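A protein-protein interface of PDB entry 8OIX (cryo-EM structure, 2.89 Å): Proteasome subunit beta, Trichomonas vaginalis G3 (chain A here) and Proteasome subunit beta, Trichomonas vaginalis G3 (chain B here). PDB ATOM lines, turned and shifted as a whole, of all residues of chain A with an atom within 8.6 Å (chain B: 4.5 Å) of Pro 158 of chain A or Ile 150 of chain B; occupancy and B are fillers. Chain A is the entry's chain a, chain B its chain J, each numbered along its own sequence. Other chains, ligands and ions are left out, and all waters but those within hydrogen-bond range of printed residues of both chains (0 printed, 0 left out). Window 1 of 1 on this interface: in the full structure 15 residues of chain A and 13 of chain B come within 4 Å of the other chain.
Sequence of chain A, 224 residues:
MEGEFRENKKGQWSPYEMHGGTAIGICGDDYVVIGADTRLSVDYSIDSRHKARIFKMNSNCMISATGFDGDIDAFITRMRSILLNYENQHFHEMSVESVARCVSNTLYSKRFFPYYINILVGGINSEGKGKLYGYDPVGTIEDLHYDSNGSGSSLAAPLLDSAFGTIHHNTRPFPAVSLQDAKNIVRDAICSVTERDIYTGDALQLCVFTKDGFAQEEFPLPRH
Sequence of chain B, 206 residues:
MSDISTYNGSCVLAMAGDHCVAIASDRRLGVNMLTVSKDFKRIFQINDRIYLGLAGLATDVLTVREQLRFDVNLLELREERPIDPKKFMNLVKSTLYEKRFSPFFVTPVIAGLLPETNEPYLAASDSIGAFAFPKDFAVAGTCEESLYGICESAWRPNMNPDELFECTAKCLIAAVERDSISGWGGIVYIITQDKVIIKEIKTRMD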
ATOM      1  N   TYR A 146      13.834 -18.306  15.891  1.00  0.00           N
ATOM      2  CA  TYR A 146      12.454 -18.681  15.641  1.00  0.00           C
ATOM      3  C   TYR A 146      11.549 -17.672  16.328  1.00  0.00           C
ATOM      4  O   TYR A 146      11.954 -16.978  17.263  1.00  0.00           O
ATOM      5  CB  TYR A 146      12.152 -20.102  16.131  1.00  0.00           C
ATOM      6  CG  TYR A 146      12.307 -20.283  17.622  1.00  0.00           C
ATOM      7  CD1 TYR A 146      11.284 -19.945  18.496  1.00  0.00           C
ATOM      8  CD2 TYR A 146      13.477 -20.798  18.155  1.00  0.00           C
ATOM      9  CE1 TYR A 146      11.423 -20.110  19.853  1.00  0.00           C
ATOM     10  CE2 TYR A 146      13.623 -20.969  19.511  1.00  0.00           C
ATOM     11  CZ  TYR A 146      12.594 -20.623  20.356  1.00  0.00           C
ATOM     12  OH  TYR A 146      12.739 -20.793  21.711  1.00  0.00           O
ATOM     13  N   SER A 148       6.954 -16.817  16.870  1.00  0.00           N
ATOM     14  CA  SER A 148       5.563 -17.129  16.604  1.00  0.00           C
ATOM     15  C   SER A 148       4.735 -15.876  16.828  1.00  0.00           C
ATOM     16  O   SER A 148       4.953 -15.144  17.798  1.00  0.00           O
ATOM     17  CB  SER A 148       5.052 -18.262  17.494  1.00  0.00           C
ATOM     18  OG  SER A 148       3.730 -18.612  17.136  1.00  0.00           O
ATOM     19  N   GLY A 152      -2.345 -17.742  17.754  1.00  0.00           N
ATOM     20  CA  GLY A 152      -1.762 -18.940  18.324  1.00  0.00           C
ATOM     21  C   GLY A 152      -0.299 -18.804  18.686  1.00  0.00           C
ATOM     22  O   GLY A 152       0.400 -19.809  18.836  1.00  0.00           O
ATOM     23  N   SER A 153       0.179 -17.564  18.815  1.00  0.00           N
ATOM     24  CA  SER A 153       1.568 -17.347  19.205  1.00  0.00           C
ATOM     25  C   SER A 153       1.862 -17.973  20.562  1.00  0.00           C
ATOM     26  O   SER A 153       2.902 -18.618  20.744  1.00  0.00           O
ATOM     27  CB  SER A 153       1.877 -15.852  19.226  1.00  0.00           C
ATOM     28  OG  SER A 153       0.955 -15.157  20.045  1.00  0.00           O
ATOM     29  N   SER A 154       0.953 -17.797  21.524  1.00  0.00           N
ATOM     30  CA  SER A 154       1.144 -18.395  22.841  1.00  0.00           C
ATOM     31  C   SER A 154       1.135 -19.913  22.760  1.00  0.00           C
ATOM     32  O   SER A 154       1.856 -20.586  23.502  1.00  0.00           O
ATOM     33  CB  SER A 154       0.064 -17.901  23.803  1.00  0.00           C
ATOM     34  OG  SER A 154       0.171 -16.504  24.015  1.00  0.00           O
ATOM     35  N   LEU A 155       0.301 -20.471  21.882  1.00  0.00           N
ATOM     36  CA  LEU A 155       0.281 -21.917  21.685  1.00  0.00           C
ATOM     37  C   LEU A 155       1.574 -22.401  21.042  1.00  0.00           C
ATOM     38  O   LEU A 155       2.192 -23.365  21.506  1.00  0.00           O
ATOM     39  CB  LEU A 155      -0.916 -22.302  20.819  1.00  0.00           C
ATOM     40  CG  LEU A 155      -2.306 -22.106  21.414  1.00  0.00           C
ATOM     41  CD1 LEU A 155      -3.288 -21.803  20.314  1.00  0.00           C
ATOM     42  CD2 LEU A 155      -2.735 -23.345  22.157  1.00  0.00           C
ATOM     43  N   ALA A 156       1.994 -21.739  19.965  1.00  0.00           N
ATOM     44  CA  ALA A 156       3.086 -22.237  19.140  1.00  0.00           C
ATOM     45  C   ALA A 156       4.458 -22.006  19.755  1.00  0.00           C
ATOM     46  O   ALA A 156       5.391 -22.760  19.460  1.00  0.00           O
ATOM     47  CB  ALA A 156       3.031 -21.583  17.764  1.00  0.00           C
ATOM     48  N   ALA A 157       4.613 -20.971  20.577  1.00  0.00           N
ATOM     49  CA  ALA A 157       5.935 -20.655  21.114  1.00  0.00           C
ATOM     50  C   ALA A 157       6.531 -21.789  21.943  1.00  0.00           C
ATOM     51  O   ALA A 157       7.718 -22.103  21.745  1.00  0.00           O
ATOM     52  CB  ALA A 157       5.870 -19.345  21.904  1.00  0.00           C
ATOM     53  N   PRO A 158       5.809 -22.426  22.874  1.00  0.00           N
ATOM     54  CA  PRO A 158       6.379 -23.603  23.549  1.00  0.00           C
ATOM     55  C   PRO A 158       6.759 -24.723  22.603  1.00  0.00           C
ATOM     56  O   PRO A 158       7.713 -25.453  22.885  1.00  0.00           O
ATOM     57  CB  PRO A 158       5.263 -24.037  24.504  1.00  0.00           C
ATOM     58  CG  PRO A 158       4.499 -22.823  24.750  1.00  0.00           C
ATOM     59  CD  PRO A 158       4.538 -22.021  23.495  1.00  0.00           C
ATOM     60  N   LEU A 159       6.029 -24.899  21.502  1.00  0.00           N
ATOM     61  CA  LEU A 159       6.398 -25.920  20.528  1.00  0.00           C
ATOM     62  C   LEU A 159       7.801 -25.675  19.992  1.00  0.00           C
ATOM     63  O   LEU A 159       8.632 -26.590  19.941  1.00  0.00           O
ATOM     64  CB  LEU A 159       5.380 -25.935  19.391  1.00  0.00           C
ATOM     65  CG  LEU A 159       3.990 -26.310  19.884  1.00  0.00           C
ATOM     66  CD1 LEU A 159       2.930 -26.046  18.836  1.00  0.00           C
ATOM     67  CD2 LEU A 159       4.028 -27.764  20.251  1.00  0.00           C
ATOM     68  N   LEU A 160       8.091 -24.430  19.620  1.00  0.00           N
ATOM     69  CA  LEU A 160       9.414 -24.100  19.110  1.00  0.00           C
ATOM     70  C   LEU A 160      10.460 -24.157  20.215  1.00  0.00           C
ATOM     71  O   LEU A 160      11.593 -24.593  19.984  1.00  0.00           O
ATOM     72  CB  LEU A 160       9.383 -22.722  18.460  1.00  0.00           C
ATOM     73  CG  LEU A 160       8.301 -22.536  17.398  1.00  0.00           C
ATOM     74  CD1 LEU A 160       8.135 -21.067  17.051  1.00  0.00           C
ATOM     75  CD2 LEU A 160       8.634 -23.352  16.165  1.00  0.00           C
ATOM     76  N   ASP A 161      10.098 -23.723  21.425  1.00  0.00           N
ATOM     77  CA  ASP A 161      11.026 -23.813  22.547  1.00  0.00           C
ATOM     78  C   ASP A 161      11.432 -25.256  22.806  1.00  0.00           C
ATOM     79  O   ASP A 161      12.607 -25.544  23.051  1.00  0.00           O
ATOM     80  CB  ASP A 161      10.403 -23.207  23.802  1.00  0.00           C
ATOM     81  CG  ASP A 161      10.033 -21.757  23.621  1.00  0.00           C
ATOM     82  OD1 ASP A 161      10.359 -21.187  22.562  1.00  0.00           O
ATOM     83  OD2 ASP A 161       9.424 -21.184  24.543  1.00  0.00           O
ATOM     84  N   SER A 162      10.472 -26.177  22.760  1.00  0.00           N
ATOM     85  CA  SER A 162      10.799 -27.586  22.926  1.00  0.00           C
ATOM     86  C   SER A 162      11.634 -28.094  21.761  1.00  0.00           C
ATOM     87  O   SER A 162      12.628 -28.799  21.967  1.00  0.00           O
ATOM     88  CB  SER A 162       9.520 -28.406  23.073  1.00  0.00           C
ATOM     89  OG  SER A 162       8.739 -27.917  24.145  1.00  0.00           O
ATOM     90  N   ALA A 163      11.258 -27.732  20.533  1.00  0.00           N
ATOM     91  CA  ALA A 163      12.000 -28.198  19.367  1.00  0.00           C
ATOM     92  C   ALA A 163      13.454 -27.747  19.399  1.00  0.00           C
ATOM     93  O   ALA A 163      14.333 -28.463  18.905  1.00  0.00           O
ATOM     94  CB  ALA A 163      11.321 -27.714  18.087  1.00  0.00           C
ATOM     95  N   PHE A 164      13.735 -26.574  19.968  1.00  0.00           N
ATOM     96  CA  PHE A 164      15.082 -26.024  19.940  1.00  0.00           C
ATOM     97  C   PHE A 164      15.716 -25.802  21.305  1.00  0.00           C
ATOM     98  O   PHE A 164      16.949 -25.789  21.390  1.00  0.00           O
ATOM     99  CB  PHE A 164      15.096 -24.698  19.166  1.00  0.00           C
ATOM    100  CG  PHE A 164      14.449 -24.787  17.816  1.00  0.00           C
ATOM    101  CD1 PHE A 164      15.024 -25.539  16.810  1.00  0.00           C
ATOM    102  CD2 PHE A 164      13.267 -24.121  17.553  1.00  0.00           C
ATOM    103  CE1 PHE A 164      14.430 -25.625  15.570  1.00  0.00           C
ATOM    104  CE2 PHE A 164      12.671 -24.206  16.315  1.00  0.00           C
ATOM    105  CZ  PHE A 164      13.256 -24.958  15.323  1.00  0.00           C
ATOM    106  N   GLY A 165      14.933 -25.632  22.367  1.00  0.00           N
ATOM    107  CA  GLY A 165      15.513 -25.382  23.673  1.00  0.00           C
ATOM    108  C   GLY A 165      16.126 -24.015  23.852  1.00  0.00           C
ATOM    109  O   GLY A 165      16.828 -23.794  24.843  1.00  0.00           O
ATOM    110  N   THR A 166      15.889 -23.088  22.920  1.00  0.00           N
ATOM    111  CA  THR A 166      16.527 -21.778  23.000  1.00  0.00           C
ATOM    112  C   THR A 166      16.009 -20.977  24.188  1.00  0.00           C
ATOM    113  O   THR A 166      16.781 -20.280  24.855  1.00  0.00           O
ATOM    114  CB  THR A 166      16.310 -21.011  21.696  1.00  0.00           C
ATOM    115  OG1 THR A 166      16.802 -21.791  20.599  1.00  0.00           O
ATOM    116  CG2 THR A 166      17.042 -19.677  21.728  1.00  0.00           C
ATOM    117  N   ILE A 167      14.709 -21.060  24.470  1.00  0.00           N
ATOM    118  CA  ILE A 167      14.169 -20.363  25.632  1.00  0.00           C
ATOM    119  C   ILE A 167      14.645 -21.026  26.918  1.00  0.00           C
ATOM    120  O   ILE A 167      14.969 -20.348  27.900  1.00  0.00           O
ATOM    121  CB  ILE A 167      12.633 -20.303  25.552  1.00  0.00           C
ATOM    122  CG1 ILE A 167      12.197 -19.340  24.448  1.00  0.00           C
ATOM    123  CG2 ILE A 167      12.041 -19.865  26.880  1.00  0.00           C
ATOM    124  CD1 ILE A 167      12.420 -17.890  24.762  1.00  0.00           C
ATOM    125  N   ILE A 185       8.717 -29.023  11.595  1.00  0.00           N
ATOM    126  CA  ILE A 185       8.420 -28.419  12.891  1.00  0.00           C
ATOM    127  C   ILE A 185       7.365 -27.336  12.738  1.00  0.00           C
ATOM    128  O   ILE A 185       6.421 -27.254  13.532  1.00  0.00           O
ATOM    129  CB  ILE A 185       9.701 -27.864  13.540  1.00  0.00           C
ATOM    130  CG1 ILE A 185      10.643 -28.995  13.947  1.00  0.00           C
ATOM    131  CG2 ILE A 185       9.359 -27.008  14.749  1.00  0.00           C
ATOM    132  CD1 ILE A 185      12.047 -28.525  14.242  1.00  0.00           C
ATOM    133  N   ASP A 188       3.976 -29.035  12.042  1.00  0.00           N
ATOM    134  CA  ASP A 188       3.407 -29.658  13.231  1.00  0.00           C
ATOM    135  C   ASP A 188       2.915 -28.610  14.219  1.00  0.00           C
ATOM    136  O   ASP A 188       1.843 -28.765  14.819  1.00  0.00           O
ATOM    137  CB  ASP A 188       4.446 -30.571  13.883  1.00  0.00           C
ATOM    138  CG  ASP A 188       4.072 -30.964  15.296  1.00  0.00           C
ATOM    139  OD1 ASP A 188       3.315 -31.943  15.464  1.00  0.00           O
ATOM    140  OD2 ASP A 188       4.540 -30.295  16.240  1.00  0.00           O
ATOM    141  N   ALA A 189       3.683 -27.537  14.403  1.00  0.00           N
ATOM    142  CA  ALA A 189       3.267 -26.477  15.310  1.00  0.00           C
ATOM    143  C   ALA A 189       2.015 -25.775  14.802  1.00  0.00           C
ATOM    144  O   ALA A 189       1.108 -25.473  15.585  1.00  0.00           O
ATOM    145  CB  ALA A 189       4.415 -25.493  15.513  1.00  0.00           C
ATOM    146  N   SER A 192      -0.909 -28.074  15.460  1.00  0.00           N
ATOM    147  CA  SER A 192      -1.305 -28.029  16.864  1.00  0.00           C
ATOM    148  C   SER A 192      -2.066 -26.748  17.182  1.00  0.00           C
ATOM    149  O   SER A 192      -3.089 -26.775  17.882  1.00  0.00           O
ATOM    150  CB  SER A 192      -0.071 -28.153  17.756  1.00  0.00           C
ATOM    151  OG  SER A 192       0.709 -29.273  17.383  1.00  0.00           O
ATOM    152  N   VAL A 193      -1.587 -25.615  16.664  1.00  0.00           N
ATOM    153  CA  VAL A 193      -2.282 -24.348  16.866  1.00  0.00           C
ATOM    154  C   VAL A 193      -3.675 -24.408  16.255  1.00  0.00           C
ATOM    155  O   VAL A 193      -4.661 -23.981  16.866  1.00  0.00           O
ATOM    156  CB  VAL A 193      -1.454 -23.186  16.294  1.00  0.00           C
ATOM    157  CG1 VAL A 193      -2.235 -21.909  16.373  1.00  0.00           C
ATOM    158  CG2 VAL A 193      -0.159 -23.042  17.058  1.00  0.00           C
ATOM    159  N   ARG A 196      -5.938 -26.149  18.424  1.00  0.00           N
ATOM    160  CA  ARG A 196      -6.275 -25.429  19.645  1.00  0.00           C
ATOM    161  C   ARG A 196      -6.788 -24.014  19.397  1.00  0.00           C
ATOM    162  O   ARG A 196      -7.804 -23.623  19.975  1.00  0.00           O
ATOM    163  CB  ARG A 196      -5.062 -25.402  20.578  1.00  0.00           C
ATOM    164  CG  ARG A 196      -4.681 -26.780  21.079  1.00  0.00           C
ATOM    165  CD  ARG A 196      -5.753 -27.313  22.012  1.00  0.00           C
ATOM    166  NE  ARG A 196      -5.668 -28.757  22.194  1.00  0.00           N
ATOM    167  CZ  ARG A 196      -6.464 -29.455  22.991  1.00  0.00           C
ATOM    168  NH1 ARG A 196      -7.408 -28.870  23.710  1.00  0.00           N
ATOM    169  NH2 ARG A 196      -6.314 -30.774  23.065  1.00  0.00           N
ATOM    170  N   SER B 146      -0.138 -21.885  26.360  1.00  0.00           N
ATOM    171  CA  SER B 146       1.165 -22.507  26.158  1.00  0.00           C
ATOM    172  C   SER B 146       1.101 -24.012  26.383  1.00  0.00           C
ATOM    173  O   SER B 146       1.629 -24.793  25.579  1.00  0.00           O
ATOM    174  CB  SER B 146       2.187 -21.866  27.095  1.00  0.00           C
ATOM    175  OG  SER B 146       2.417 -20.514  26.748  1.00  0.00           O
ATOM    176  N   LEU B 147       0.450 -24.435  27.470  1.00  0.00           N
ATOM    177  CA  LEU B 147       0.324 -25.861  27.755  1.00  0.00           C
ATOM    178  C   LEU B 147      -0.486 -26.577  26.686  1.00  0.00           C
ATOM    179  O   LEU B 147      -0.108 -27.668  26.245  1.00  0.00           O
ATOM    180  CB  LEU B 147      -0.305 -26.072  29.130  1.00  0.00           C
ATOM    181  CG  LEU B 147       0.637 -26.391  30.287  1.00  0.00           C
ATOM    182  CD1 LEU B 147      -0.147 -26.655  31.553  1.00  0.00           C
ATOM    183  CD2 LEU B 147       1.511 -27.580  29.939  1.00  0.00           C
ATOM    184  N   TYR B 148      -1.612 -25.993  26.266  1.00  0.00           N
ATOM    185  CA  TYR B 148      -2.396 -26.597  25.194  1.00  0.00           C
ATOM    186  C   TYR B 148      -1.543 -26.793  23.952  1.00  0.00           C
ATOM    187  O   TYR B 148      -1.507 -27.886  23.372  1.00  0.00           O
ATOM    188  CB  TYR B 148      -3.616 -25.735  24.862  1.00  0.00           C
ATOM    189  CG  TYR B 148      -4.826 -25.980  25.733  1.00  0.00           C
ATOM    190  CD1 TYR B 148      -5.392 -27.243  25.826  1.00  0.00           C
ATOM    191  CD2 TYR B 148      -5.430 -24.940  26.425  1.00  0.00           C
ATOM    192  CE1 TYR B 148      -6.504 -27.469  26.611  1.00  0.00           C
ATOM    193  CE2 TYR B 148      -6.545 -25.155  27.208  1.00  0.00           C
ATOM    194  CZ  TYR B 148      -7.076 -26.423  27.300  1.00  0.00           C
ATOM    195  OH  TYR B 148      -8.184 -26.644  28.082  1.00  0.00           O
ATOM    196  N   GLY B 149      -0.827 -25.743  23.545  1.00  0.00           N
ATOM    197  CA  GLY B 149      -0.020 -25.834  22.342  1.00  0.00           C
ATOM    198  C   GLY B 149       1.040 -26.911  22.431  1.00  0.00           C
ATOM    199  O   GLY B 149       1.177 -27.737  21.526  1.00  0.00           O
ATOM    200  N   ILE B 150       1.792 -26.935  23.535  1.00  0.00           N
ATOM    201  CA  ILE B 150       2.903 -27.879  23.620  1.00  0.00           C
ATOM    202  C   ILE B 150       2.390 -29.309  23.753  1.00  0.00           C
ATOM    203  O   ILE B 150       2.926 -30.233  23.126  1.00  0.00           O
ATOM    204  CB  ILE B 150       3.864 -27.503  24.765  1.00  0.00           C
ATOM    205  CG1 ILE B 150       5.057 -28.461  24.789  1.00  0.00           C
ATOM    206  CG2 ILE B 150       3.161 -27.509  26.111  1.00  0.00           C
ATOM    207  CD1 ILE B 150       5.744 -28.613  23.454  1.00  0.00           C
ATOM    208  N   CYS B 151       1.337 -29.519  24.544  1.00  0.00           N
ATOM    209  CA  CYS B 151       0.852 -30.872  24.779  1.00  0.00           C
ATOM    210  C   CYS B 151       0.096 -31.431  23.582  1.00  0.00           C
ATOM    211  O   CYS B 151       0.050 -32.653  23.407  1.00  0.00           O
ATOM    212  CB  CYS B 151      -0.021 -30.897  26.029  1.00  0.00           C
ATOM    213  SG  CYS B 151       0.864 -30.441  27.529  1.00  0.00           S
ATOM    214  N   GLU B 152      -0.511 -30.573  22.756  1.00  0.00           N
ATOM    215  CA  GLU B 152      -1.183 -31.077  21.564  1.00  0.00           C
ATOM    216  C   GLU B 152      -0.208 -31.792  20.639  1.00  0.00           C
ATOM    217  O   GLU B 152      -0.503 -32.880  20.132  1.00  0.00           O
ATOM    218  CB  GLU B 152      -1.877 -29.929  20.831  1.00  0.00           C
ATOM    219  CG  GLU B 152      -2.732 -30.366  19.651  1.00  0.00           C
ATOM    220  CD  GLU B 152      -4.028 -31.031  20.074  1.00  0.00           C
ATOM    221  OE1 GLU B 152      -4.304 -31.100  21.290  1.00  0.00           O
ATOM    222  OE2 GLU B 152      -4.774 -31.494  19.185  1.00  0.00           O
ATOM    223  N   SER B 153       0.962 -31.196  20.407  1.00  0.00           N
ATOM    224  CA  SER B 153       1.969 -31.827  19.561  1.00  0.00           C
ATOM    225  C   SER B 153       2.734 -32.919  20.294  1.00  0.00           C
ATOM    226  O   SER B 153       3.053 -33.958  19.703  1.00  0.00           O
ATOM    227  CB  SER B 153       2.944 -30.780  19.033  1.00  0.00           C
ATOM    228  OG  SER B 153       3.997 -31.387  18.305  1.00  0.00           O
ATOM    229  N   ALA B 154       3.041 -32.708  21.573  1.00  0.00           N
ATOM    230  CA  ALA B 154       4.004 -33.562  22.254  1.00  0.00           C
ATOM    231  C   ALA B 154       3.382 -34.820  22.846  1.00  0.00           C
ATOM    232  O   ALA B 154       4.014 -35.880  22.828  1.00  0.00           O
ATOM    233  CB  ALA B 154       4.715 -32.768  23.348  1.00  0.00           C
ATOM    234  N   CYS B 171       7.061 -30.628  28.563  1.00  0.00           N
ATOM    235  CA  CYS B 171       5.922 -29.856  28.105  1.00  0.00           C
ATOM    236  C   CYS B 171       5.536 -28.779  29.123  1.00  0.00           C
ATOM    237  O   CYS B 171       5.270 -27.628  28.747  1.00  0.00           O
ATOM    238  CB  CYS B 171       4.787 -30.854  27.802  1.00  0.00           C
ATOM    239  SG  CYS B 171       5.350 -32.247  26.644  1.00  0.00           S
ATOM    240  N   ALA B 174       8.259 -26.084  28.902  1.00  0.00           N
ATOM    241  CA  ALA B 174       8.025 -25.227  27.747  1.00  0.00           C
ATOM    242  C   ALA B 174       6.896 -24.246  28.020  1.00  0.00           C
ATOM    243  O   ALA B 174       6.965 -23.079  27.618  1.00  0.00           O
ATOM    244  CB  ALA B 174       7.714 -26.076  26.517  1.00  0.00           C
ATOM    245  N   ALA B 175       5.841 -24.703  28.696  1.00  0.00           N
ATOM    246  CA  ALA B 175       4.732 -23.808  29.010  1.00  0.00           C
ATOM    247  C   ALA B 175       5.157 -22.712  29.983  1.00  0.00           C
ATOM    248  O   ALA B 175       4.889 -21.527  29.751  1.00  0.00           O
ATOM    249  CB  ALA B 175       3.563 -24.605  29.579  1.00  0.00           C
ATOM    250  N   ARG B 178       7.381 -19.797  28.791  1.00  0.00           N
ATOM    251  CA  ARG B 178       6.727 -18.760  28.011  1.00  0.00           C
ATOM    252  C   ARG B 178       5.720 -17.961  28.821  1.00  0.00           C
ATOM    253  O   ARG B 178       5.145 -17.003  28.298  1.00  0.00           O
ATOM    254  CB  ARG B 178       6.038 -19.370  26.790  1.00  0.00           C
ATOM    255  CG  ARG B 178       6.990 -19.673  25.660  1.00  0.00           C
ATOM    256  CD  ARG B 178       7.590 -18.400  25.098  1.00  0.00           C
ATOM    257  NE  ARG B 178       8.368 -18.646  23.891  1.00  0.00           N
ATOM    258  CZ  ARG B 178       8.843 -17.694  23.099  1.00  0.00           C
ATOM    259  NH1 ARG B 178       8.639 -16.415  23.360  1.00  0.00           N
ATOM    260  NH2 ARG B 178       9.539 -18.037  22.019  1.00  0.00           N
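The backbone carbonyl oxygen (O) of Ser 154 of chain A sits at hydrogen-bond distance from the side-chain hydroxyl (OG) of Ser 146 of chain B. OE1 of Glu 152 of chain B lies within salt-bridge range of NH2 of Arg 196 of chain A (2.7 Å). OG of Ser 153 of chain B lies within hydrogen-bond range of OD1 of Asp 188 of chain A (3.0 Å). NE of Arg 178 of chain B lies within salt-bridge range of OD2 of Asp 161 of chain A, 2.8 Å away.
OH of Tyr 146 of chain A is in hydrogen-bond range of OD1 of Asp 161 of chain A (2.6 Å). The side-chain hydroxyl (OH) of Tyr 146 of chain A lies close to the backbone NH (N) of Ile 167 of chain A (3.4 Å). O of Pro 158 of chain A is in hydrogen-bond range of OG of Ser 162 of chain A (3.0 Å). O of Asp 188 of chain A is in hydrogen-bond range of OG of Ser 192 of chain A.
Tyr 146 of chain A touches Arg 178 of chain B. Tyr 148 of chain B touches Leu 155 of chain A. Gly 149 of chain B touches Leu 155 of chain A. NE of Arg 178 of chain B touches CB of Ala 157 of chain A (3.3 Å). Pro 158 of chain A touches Ser 146 of chain B. Pro 158 of chain A touches Ala 174 of chain B. CB of Ser 153 of chain B touches CD2 of Leu 159 of chain A (3.4 Å). Ser 192 of chain A touches Gly 149 of chain B (CB to O, 3.99 Å). Ser 153 of chain B touches Ser 192 of chain A (CB to OG, 3.2 Å). Tyr 148 of chain B touches Arg 196 of chain A.
Of the printed residues of chain B, Tyr 146 of chain A touches Arg 178. Of the printed residues of chain B, Asp 161 of chain A touches Arg 178 (2.8 Å). Gly 165 of chain A touches none of the printed residues of chain B. Ile 185 of chain A touches none of the printed residues of chain B. Of the printed residues of chain A, Tyr 148 of chain B touches Leu 155 (3.7 Å) and Arg 196 (3.3 Å). Ile 150 of chain B touches three residues of chain A. Printed residues of chain A within 4 Å of Glu 152 of chain B: Ser 192 (3.9 Å) and Arg 196 (2.7 Å). Of the printed residues of chain A, Ala 174 of chain B touches Pro 158 and Ser 162. The nearest residue of chain B that does not touch Pro 158 of chain A is Arg 178 of chain B (4.03 Å). The nearest residue of chain A that does not touch Ile 150 of chain B is Leu 155 of chain A (4.1 Å).
Along chain B the printed residues that touch a printed residue of chain A span positions 146 to 178. Printed residues of chain A that touch a printed residue of chain B: Tyr 146, Ser 154, Leu 155, Ala 157, Pro 158, Leu 159, Asp 161, Ser 162, Ile 167, Asp 188, Ser 192 and Arg 196. Hydrophobic or aromatic side chains of chain A that line the printed part of chain B: Tyr 146, Leu 155, Ala 157, Pro 158, Leu 159 and Ile 167. Along chain A the printed residues that touch a printed residue of chain B span positions 146 to 196.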
